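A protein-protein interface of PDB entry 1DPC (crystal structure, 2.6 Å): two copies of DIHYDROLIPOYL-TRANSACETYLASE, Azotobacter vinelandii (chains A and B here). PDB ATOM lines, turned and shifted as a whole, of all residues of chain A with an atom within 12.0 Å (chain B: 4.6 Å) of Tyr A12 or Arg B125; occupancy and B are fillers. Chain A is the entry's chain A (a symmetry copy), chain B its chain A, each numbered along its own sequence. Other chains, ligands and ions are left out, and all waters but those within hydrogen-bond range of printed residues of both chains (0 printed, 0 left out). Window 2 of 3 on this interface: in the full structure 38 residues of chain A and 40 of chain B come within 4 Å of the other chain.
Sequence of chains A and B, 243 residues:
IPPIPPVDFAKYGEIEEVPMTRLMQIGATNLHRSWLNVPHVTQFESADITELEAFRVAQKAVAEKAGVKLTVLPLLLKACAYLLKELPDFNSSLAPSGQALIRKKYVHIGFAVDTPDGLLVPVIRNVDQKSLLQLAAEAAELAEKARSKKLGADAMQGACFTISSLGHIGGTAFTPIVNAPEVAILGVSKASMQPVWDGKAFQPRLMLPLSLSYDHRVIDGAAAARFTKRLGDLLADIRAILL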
ATOM      1  N   PRO A   5      -4.594  -9.279 -20.962  1.00  0.00           N
ATOM      2  CA  PRO A   5      -3.436  -8.480 -21.348  1.00  0.00           C
ATOM      3  C   PRO A   5      -2.500  -9.117 -22.383  1.00  0.00           C
ATOM      4  O   PRO A   5      -2.137 -10.297 -22.267  1.00  0.00           O
ATOM      5  CB  PRO A   5      -2.770  -8.196 -20.017  1.00  0.00           C
ATOM      6  CG  PRO A   5      -3.940  -8.112 -19.060  1.00  0.00           C
ATOM      7  CD  PRO A   5      -4.731  -9.316 -19.504  1.00  0.00           C
ATOM      8  N   PRO A   6      -2.091  -8.374 -23.419  1.00  0.00           N
ATOM      9  CA  PRO A   6      -1.193  -8.852 -24.465  1.00  0.00           C
ATOM     10  C   PRO A   6       0.218  -8.970 -23.923  1.00  0.00           C
ATOM     11  O   PRO A   6       0.656  -8.171 -23.086  1.00  0.00           O
ATOM     12  CB  PRO A   6      -1.345  -7.834 -25.566  1.00  0.00           C
ATOM     13  CG  PRO A   6      -1.528  -6.551 -24.778  1.00  0.00           C
ATOM     14  CD  PRO A   6      -2.483  -6.993 -23.668  1.00  0.00           C
ATOM     15  N   VAL A   7       0.944  -9.964 -24.411  1.00  0.00           N
ATOM     16  CA  VAL A   7       2.281 -10.226 -23.919  1.00  0.00           C
ATOM     17  C   VAL A   7       3.170 -10.263 -25.136  1.00  0.00           C
ATOM     18  O   VAL A   7       2.780 -10.792 -26.179  1.00  0.00           O
ATOM     19  CB  VAL A   7       2.315 -11.574 -23.185  1.00  0.00           C
ATOM     20  CG1 VAL A   7       3.694 -11.768 -22.622  1.00  0.00           C
ATOM     21  CG2 VAL A   7       1.289 -11.628 -22.051  1.00  0.00           C
ATOM     22  N   ASP A   8       4.370  -9.707 -25.049  1.00  0.00           N
ATOM     23  CA  ASP A   8       5.277  -9.718 -26.185  1.00  0.00           C
ATOM     24  C   ASP A   8       5.991 -11.074 -26.063  1.00  0.00           C
ATOM     25  O   ASP A   8       7.069 -11.181 -25.477  1.00  0.00           O
ATOM     26  CB  ASP A   8       6.206  -8.460 -26.037  1.00  0.00           C
ATOM     27  CG  ASP A   8       7.088  -7.970 -27.218  1.00  0.00           C
ATOM     28  OD1 ASP A   8       8.151  -8.550 -27.477  1.00  0.00           O
ATOM     29  OD2 ASP A   8       6.716  -6.981 -27.875  1.00  0.00           O
ATOM     30  N   PHE A   9       5.424 -12.149 -26.611  1.00  0.00           N
ATOM     31  CA  PHE A   9       5.998 -13.482 -26.440  1.00  0.00           C
ATOM     32  C   PHE A   9       7.413 -13.687 -26.896  1.00  0.00           C
ATOM     33  O   PHE A   9       8.161 -14.492 -26.346  1.00  0.00           O
ATOM     34  CB  PHE A   9       5.110 -14.514 -27.123  1.00  0.00           C
ATOM     35  CG  PHE A   9       3.798 -14.611 -26.351  1.00  0.00           C
ATOM     36  CD1 PHE A   9       3.808 -14.948 -24.985  1.00  0.00           C
ATOM     37  CD2 PHE A   9       2.595 -14.305 -26.989  1.00  0.00           C
ATOM     38  CE1 PHE A   9       2.609 -14.968 -24.277  1.00  0.00           C
ATOM     39  CE2 PHE A   9       1.407 -14.334 -26.267  1.00  0.00           C
ATOM     40  CZ  PHE A   9       1.415 -14.663 -24.918  1.00  0.00           C
ATOM     41  N   ALA A  10       7.806 -12.842 -27.837  1.00  0.00           N
ATOM     42  CA  ALA A  10       9.138 -12.906 -28.354  1.00  0.00           C
ATOM     43  C   ALA A  10      10.173 -12.386 -27.385  1.00  0.00           C
ATOM     44  O   ALA A  10      11.351 -12.608 -27.638  1.00  0.00           O
ATOM     45  CB  ALA A  10       9.205 -12.119 -29.625  1.00  0.00           C
ATOM     46  N   LYS A  11       9.851 -11.741 -26.253  1.00  0.00           N
ATOM     47  CA  LYS A  11      10.895 -11.334 -25.305  1.00  0.00           C
ATOM     48  C   LYS A  11      11.587 -12.559 -24.710  1.00  0.00           C
ATOM     49  O   LYS A  11      12.738 -12.515 -24.252  1.00  0.00           O
ATOM     50  CB  LYS A  11      10.381 -10.566 -24.091  1.00  0.00           C
ATOM     51  CG  LYS A  11       9.631  -9.263 -24.287  1.00  0.00           C
ATOM     52  CD  LYS A  11       9.368  -8.707 -22.891  1.00  0.00           C
ATOM     53  CE  LYS A  11       8.342  -7.570 -22.888  1.00  0.00           C
ATOM     54  NZ  LYS A  11       8.894  -6.226 -23.036  1.00  0.00           N
ATOM     55  N   TYR A  12      10.834 -13.667 -24.703  1.00  0.00           N
ATOM     56  CA  TYR A  12      11.270 -14.892 -24.071  1.00  0.00           C
ATOM     57  C   TYR A  12      11.890 -15.893 -25.026  1.00  0.00           C
ATOM     58  O   TYR A  12      12.414 -16.922 -24.585  1.00  0.00           O
ATOM     59  CB  TYR A  12      10.060 -15.472 -23.369  1.00  0.00           C
ATOM     60  CG  TYR A  12       9.437 -14.452 -22.439  1.00  0.00           C
ATOM     61  CD1 TYR A  12      10.162 -14.029 -21.329  1.00  0.00           C
ATOM     62  CD2 TYR A  12       8.170 -13.936 -22.701  1.00  0.00           C
ATOM     63  CE1 TYR A  12       9.639 -13.064 -20.476  1.00  0.00           C
ATOM     64  CE2 TYR A  12       7.636 -12.966 -21.841  1.00  0.00           C
ATOM     65  CZ  TYR A  12       8.383 -12.532 -20.739  1.00  0.00           C
ATOM     66  OH  TYR A  12       7.907 -11.570 -19.860  1.00  0.00           O
ATOM     67  N   GLY A  13      11.814 -15.652 -26.326  1.00  0.00           N
ATOM     68  CA  GLY A  13      12.368 -16.570 -27.286  1.00  0.00           C
ATOM     69  C   GLY A  13      11.744 -16.393 -28.650  1.00  0.00           C
ATOM     70  O   GLY A  13      10.951 -15.491 -28.888  1.00  0.00           O
ATOM     71  N   GLU A  14      12.058 -17.328 -29.529  1.00  0.00           N
ATOM     72  CA  GLU A  14      11.663 -17.262 -30.913  1.00  0.00           C
ATOM     73  C   GLU A  14      10.207 -17.676 -30.947  1.00  0.00           C
ATOM     74  O   GLU A  14       9.849 -18.625 -30.261  1.00  0.00           O
ATOM     75  CB  GLU A  14      12.587 -18.218 -31.666  1.00  0.00           C
ATOM     76  CG  GLU A  14      13.289 -17.769 -32.958  1.00  0.00           C
ATOM     77  CD  GLU A  14      12.500 -17.945 -34.271  1.00  0.00           C
ATOM     78  OE1 GLU A  14      12.492 -19.062 -34.819  1.00  0.00           O
ATOM     79  OE2 GLU A  14      11.909 -16.963 -34.751  1.00  0.00           O
ATOM     80  N   ILE A  15       9.341 -16.996 -31.669  1.00  0.00           N
ATOM     81  CA  ILE A  15       7.948 -17.371 -31.770  1.00  0.00           C
ATOM     82  C   ILE A  15       7.679 -17.474 -33.262  1.00  0.00           C
ATOM     83  O   ILE A  15       8.431 -16.951 -34.093  1.00  0.00           O
ATOM     84  CB  ILE A  15       7.024 -16.308 -31.157  1.00  0.00           C
ATOM     85  CG1 ILE A  15       7.251 -14.974 -31.859  1.00  0.00           C
ATOM     86  CG2 ILE A  15       7.260 -16.232 -29.642  1.00  0.00           C
ATOM     87  CD1 ILE A  15       6.199 -13.874 -31.574  1.00  0.00           C
ATOM     88  N   GLU A  16       6.584 -18.108 -33.624  1.00  0.00           N
ATOM     89  CA  GLU A  16       6.190 -18.260 -35.010  1.00  0.00           C
ATOM     90  C   GLU A  16       4.671 -18.121 -35.003  1.00  0.00           C
ATOM     91  O   GLU A  16       4.033 -18.613 -34.071  1.00  0.00           O
ATOM     92  CB  GLU A  16       6.631 -19.636 -35.478  1.00  0.00           C
ATOM     93  CG  GLU A  16       6.133 -20.074 -36.856  1.00  0.00           C
ATOM     94  CD  GLU A  16       6.250 -21.564 -37.187  1.00  0.00           C
ATOM     95  OE1 GLU A  16       6.099 -22.418 -36.301  1.00  0.00           O
ATOM     96  OE2 GLU A  16       6.469 -21.865 -38.363  1.00  0.00           O
ATOM     97  N   TYR B 106      10.354 -21.998 -27.607  1.00  0.00           N
ATOM     98  CA  TYR B 106      11.147 -22.133 -26.395  1.00  0.00           C
ATOM     99  C   TYR B 106      10.305 -22.904 -25.390  1.00  0.00           C
ATOM    100  O   TYR B 106       9.085 -22.889 -25.559  1.00  0.00           O
ATOM    101  CB  TYR B 106      11.497 -20.727 -25.856  1.00  0.00           C
ATOM    102  CG  TYR B 106      10.341 -19.724 -25.701  1.00  0.00           C
ATOM    103  CD1 TYR B 106       9.970 -18.892 -26.768  1.00  0.00           C
ATOM    104  CD2 TYR B 106       9.662 -19.603 -24.485  1.00  0.00           C
ATOM    105  CE1 TYR B 106       8.947 -17.941 -26.610  1.00  0.00           C
ATOM    106  CE2 TYR B 106       8.645 -18.654 -24.324  1.00  0.00           C
ATOM    107  CZ  TYR B 106       8.296 -17.825 -25.391  1.00  0.00           C
ATOM    108  OH  TYR B 106       7.311 -16.892 -25.213  1.00  0.00           O
ATOM    109  N   VAL B 107      10.807 -23.570 -24.349  1.00  0.00           N
ATOM    110  CA  VAL B 107       9.927 -24.249 -23.408  1.00  0.00           C
ATOM    111  C   VAL B 107      10.253 -23.725 -22.026  1.00  0.00           C
ATOM    112  O   VAL B 107      11.317 -24.038 -21.470  1.00  0.00           O
ATOM    113  CB  VAL B 107      10.125 -25.809 -23.444  1.00  0.00           C
ATOM    114  CG1 VAL B 107       9.036 -26.413 -22.574  1.00  0.00           C
ATOM    115  CG2 VAL B 107      10.019 -26.403 -24.854  1.00  0.00           C
ATOM    116  N   HIS B 108       9.461 -22.825 -21.446  1.00  0.00           N
ATOM    117  CA  HIS B 108       9.718 -22.412 -20.069  1.00  0.00           C
ATOM    118  C   HIS B 108       8.455 -22.851 -19.347  1.00  0.00           C
ATOM    119  O   HIS B 108       7.353 -22.672 -19.889  1.00  0.00           O
ATOM    120  CB  HIS B 108       9.831 -20.931 -19.889  1.00  0.00           C
ATOM    121  CG  HIS B 108      10.771 -20.251 -20.858  1.00  0.00           C
ATOM    122  ND1 HIS B 108      10.604 -19.016 -21.282  1.00  0.00           N
ATOM    123  CD2 HIS B 108      11.897 -20.757 -21.451  1.00  0.00           C
ATOM    124  CE1 HIS B 108      11.586 -18.761 -22.098  1.00  0.00           C
ATOM    125  NE2 HIS B 108      12.357 -19.811 -22.202  1.00  0.00           N
ATOM    126  N   VAL B 123       8.901 -19.585 -12.696  1.00  0.00           N
ATOM    127  CA  VAL B 123       9.088 -20.155 -14.019  1.00  0.00           C
ATOM    128  C   VAL B 123      10.503 -20.668 -14.237  1.00  0.00           C
ATOM    129  O   VAL B 123      11.456 -19.930 -14.023  1.00  0.00           O
ATOM    130  CB  VAL B 123       8.790 -19.088 -15.083  1.00  0.00           C
ATOM    131  CG1 VAL B 123       9.083 -19.578 -16.493  1.00  0.00           C
ATOM    132  CG2 VAL B 123       7.331 -18.727 -14.974  1.00  0.00           C
ATOM    133  N   ILE B 124      10.718 -21.890 -14.715  1.00  0.00           N
ATOM    134  CA  ILE B 124      12.029 -22.405 -15.013  1.00  0.00           C
ATOM    135  C   ILE B 124      12.141 -22.283 -16.523  1.00  0.00           C
ATOM    136  O   ILE B 124      11.320 -22.756 -17.303  1.00  0.00           O
ATOM    137  CB  ILE B 124      12.126 -23.870 -14.528  1.00  0.00           C
ATOM    138  CG1 ILE B 124      12.000 -23.959 -13.015  1.00  0.00           C
ATOM    139  CG2 ILE B 124      13.465 -24.435 -14.925  1.00  0.00           C
ATOM    140  CD1 ILE B 124      11.940 -25.406 -12.513  1.00  0.00           C
ATOM    141  N   ARG B 125      13.193 -21.617 -16.948  1.00  0.00           N
ATOM    142  CA  ARG B 125      13.440 -21.323 -18.341  1.00  0.00           C
ATOM    143  C   ARG B 125      14.164 -22.483 -18.995  1.00  0.00           C
ATOM    144  O   ARG B 125      15.013 -23.113 -18.383  1.00  0.00           O
ATOM    145  CB  ARG B 125      14.310 -20.068 -18.476  1.00  0.00           C
ATOM    146  CG  ARG B 125      13.823 -18.791 -17.797  1.00  0.00           C
ATOM    147  CD  ARG B 125      12.715 -18.131 -18.600  1.00  0.00           C
ATOM    148  NE  ARG B 125      11.959 -17.160 -17.823  1.00  0.00           N
ATOM    149  CZ  ARG B 125      11.983 -15.845 -18.067  1.00  0.00           C
ATOM    150  NH1 ARG B 125      12.731 -15.302 -19.042  1.00  0.00           N
ATOM    151  NH2 ARG B 125      11.239 -15.064 -17.286  1.00  0.00           N
ATOM    152  N   ASN B 126      13.777 -22.810 -20.211  1.00  0.00           N
ATOM    153  CA  ASN B 126      14.451 -23.787 -21.045  1.00  0.00           C
ATOM    154  C   ASN B 126      14.575 -25.148 -20.382  1.00  0.00           C
ATOM    155  O   ASN B 126      15.601 -25.828 -20.416  1.00  0.00           O
ATOM    156  CB  ASN B 126      15.842 -23.307 -21.445  1.00  0.00           C
ATOM    157  CG  ASN B 126      15.789 -22.041 -22.260  1.00  0.00           C
ATOM    158  OD1 ASN B 126      15.122 -21.929 -23.291  1.00  0.00           O
ATOM    159  ND2 ASN B 126      16.458 -21.002 -21.795  1.00  0.00           N
ATOM    160  N   VAL B 127      13.420 -25.618 -19.900  1.00  0.00           N
ATOM    161  CA  VAL B 127      13.327 -26.875 -19.182  1.00  0.00           C
ATOM    162  C   VAL B 127      13.876 -27.980 -20.068  1.00  0.00           C
ATOM    163  O   VAL B 127      14.645 -28.826 -19.642  1.00  0.00           O
ATOM    164  CB  VAL B 127      11.860 -27.116 -18.823  1.00  0.00           C
ATOM    165  CG1 VAL B 127      11.717 -28.426 -18.077  1.00  0.00           C
ATOM    166  CG2 VAL B 127      11.372 -25.995 -17.941  1.00  0.00           C
ATOM    167  N   LYS B 130      17.702 -28.791 -19.531  1.00  0.00           N
ATOM    168  CA  LYS B 130      18.323 -28.978 -18.256  1.00  0.00           C
ATOM    169  C   LYS B 130      18.139 -30.407 -17.839  1.00  0.00           C
ATOM    170  O   LYS B 130      17.256 -31.100 -18.318  1.00  0.00           O
ATOM    171  CB  LYS B 130      17.698 -28.010 -17.290  1.00  0.00           C
ATOM    172  CG  LYS B 130      17.966 -26.593 -17.730  1.00  0.00           C
ATOM    173  CD  LYS B 130      17.354 -25.605 -16.750  1.00  0.00           C
ATOM    174  CE  LYS B 130      17.700 -24.202 -17.222  1.00  0.00           C
ATOM    175  NZ  LYS B 130      17.189 -23.229 -16.291  1.00  0.00           N
ATOM    176  N   GLU B 138      17.168 -26.043  -9.146  1.00  0.00           N
ATOM    177  CA  GLU B 138      16.504 -24.806  -9.502  1.00  0.00           C
ATOM    178  C   GLU B 138      15.076 -24.705  -8.971  1.00  0.00           C
ATOM    179  O   GLU B 138      14.695 -23.673  -8.400  1.00  0.00           O
ATOM    180  CB  GLU B 138      16.540 -24.723 -10.988  1.00  0.00           C
ATOM    181  CG  GLU B 138      16.337 -23.324 -11.494  1.00  0.00           C
ATOM    182  CD  GLU B 138      16.561 -23.202 -12.988  1.00  0.00           C
ATOM    183  OE1 GLU B 138      17.297 -24.006 -13.580  1.00  0.00           O
ATOM    184  OE2 GLU B 138      15.984 -22.276 -13.555  1.00  0.00           O
ATOM    185  N   ASP B 154      10.563 -10.772 -12.508  1.00  0.00           N
ATOM    186  CA  ASP B 154      11.176 -11.330 -13.691  1.00  0.00           C
ATOM    187  C   ASP B 154      10.931 -12.840 -13.777  1.00  0.00           C
ATOM    188  O   ASP B 154      10.340 -13.341 -14.730  1.00  0.00           O
ATOM    189  CB  ASP B 154      12.660 -10.997 -13.603  1.00  0.00           C
ATOM    190  CG  ASP B 154      13.537 -11.723 -14.612  1.00  0.00           C
ATOM    191  OD1 ASP B 154      13.319 -11.563 -15.816  1.00  0.00           O
ATOM    192  OD2 ASP B 154      14.432 -12.453 -14.179  1.00  0.00           O
ATOM    193  N   GLN B 157       7.714 -14.655 -15.288  1.00  0.00           N
ATOM    194  CA  GLN B 157       7.185 -14.337 -16.591  1.00  0.00           C
ATOM    195  C   GLN B 157       7.572 -15.243 -17.725  1.00  0.00           C
ATOM    196  O   GLN B 157       8.587 -15.932 -17.705  1.00  0.00           O
ATOM    197  CB  GLN B 157       7.589 -12.931 -16.916  1.00  0.00           C
ATOM    198  CG  GLN B 157       6.477 -11.955 -16.595  1.00  0.00           C
ATOM    199  CD  GLN B 157       6.893 -10.802 -15.695  1.00  0.00           C
ATOM    200  OE1 GLN B 157       6.340 -10.613 -14.611  1.00  0.00           O
ATOM    201  NE2 GLN B 157       7.841  -9.962 -16.093  1.00  0.00           N
ATOM    202  N   GLY B 158       6.703 -15.242 -18.720  1.00  0.00           N
ATOM    203  CA  GLY B 158       6.975 -15.900 -19.980  1.00  0.00           C
ATOM    204  C   GLY B 158       6.995 -17.409 -19.961  1.00  0.00           C
ATOM    205  O   GLY B 158       7.786 -18.046 -20.676  1.00  0.00           O
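The side-chain hydroxyl of Tyr B106 lies within hydrogen-bond range of the backbone carbonyl oxygen of Phe A9, at 2.8 Å.
A ring nitrogen (ND1) of His B108 is in hydrogen-bond range of the backbone carbonyl oxygen of Gly B158 (3.0 Å).
The side-chain amino group of Lys B130 lies within hydrogen-bond range of the backbone carbonyl oxygen of Arg B125, at 3.0 Å.
NH2 of Arg B125 sits at hydrogen-bond distance from O of Asp B154, 3.2 Å away.
NH2 of Arg B125 sits at hydrogen-bond distance from O of Gln B157 (2.8 Å).
CZ of Tyr B106 touches CB of Tyr A12 (3.6 Å).
O of Tyr A12 touches CE1 of His B108 (3.2 Å).
CD1 of Tyr A12 touches NH1 of Arg B125 (3.7 Å).
CB of Gln B157 touches OH of Tyr A12, at 3.3 Å.
CA of Gly B158 touches CE2 of Tyr A12 (3.5 Å).
Tyr B106 touches Gly A13 (CD1 to CA, 3.4 Å).
Tyr B106 touches Glu A14 (CD1 to O, 3.5 Å).
Ile A15 touches Tyr B106 (CG2 to CE1, 3.9 Å).
Of chain B, only Tyr B106, His B108, Arg B125, Gln B157 and Gly B158 come within 4 Å of Tyr A12.
Of the printed residues of chain A, Arg B125 touches Tyr A12.
Of the printed residues of chain A, Tyr B106 touches Phe A9 (2.8 Å), Tyr A12 (3.6 Å), Gly A13 (3.4 Å), Glu A14 (3.5 Å) and Ile A15 (3.9 Å).
Printed residues of chain A within 4 Å of His B108: Tyr A12.
No residue of chain A comes within 4 Å of Val B123.
No residue of chain A comes within 4 Å of Ile B124.
No residue of chain A comes within 4 Å of Asp B154.
Gln B157 touches just one residue of chain A: Tyr A12.
Gly B158 touches just one residue of chain A: Tyr A12.
Of the printed residues of chain B, Phe A9 touches Tyr B106.
Printed residues of chain B within 4 Å of Gly A13: Tyr B106.
Of the printed residues of chain B, Glu A14 touches Tyr B106 (3.5 Å).
Of the printed residues of chain B, Ile A15 touches Tyr B106 (3.9 Å).
Val B107 touches none of the printed residues of chain A.
The nearest printed residue of chain B that does not touch Tyr A12 is Asp B154 (5.8 Å).
Of the 13 printed residues of chain B, 5 touch a printed residue of chain A.
Hydrophobic or aromatic side chains of chain B that line the printed part of chain A: Tyr B106 and His B108.
Along chain B the printed residues that touch a printed residue of chain A span positions 106 to 158.
No position is printed for both chains.
Of the 9 pairs that touch across the chains among the printed residues, none has its exchanged pair printed and touching as well.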
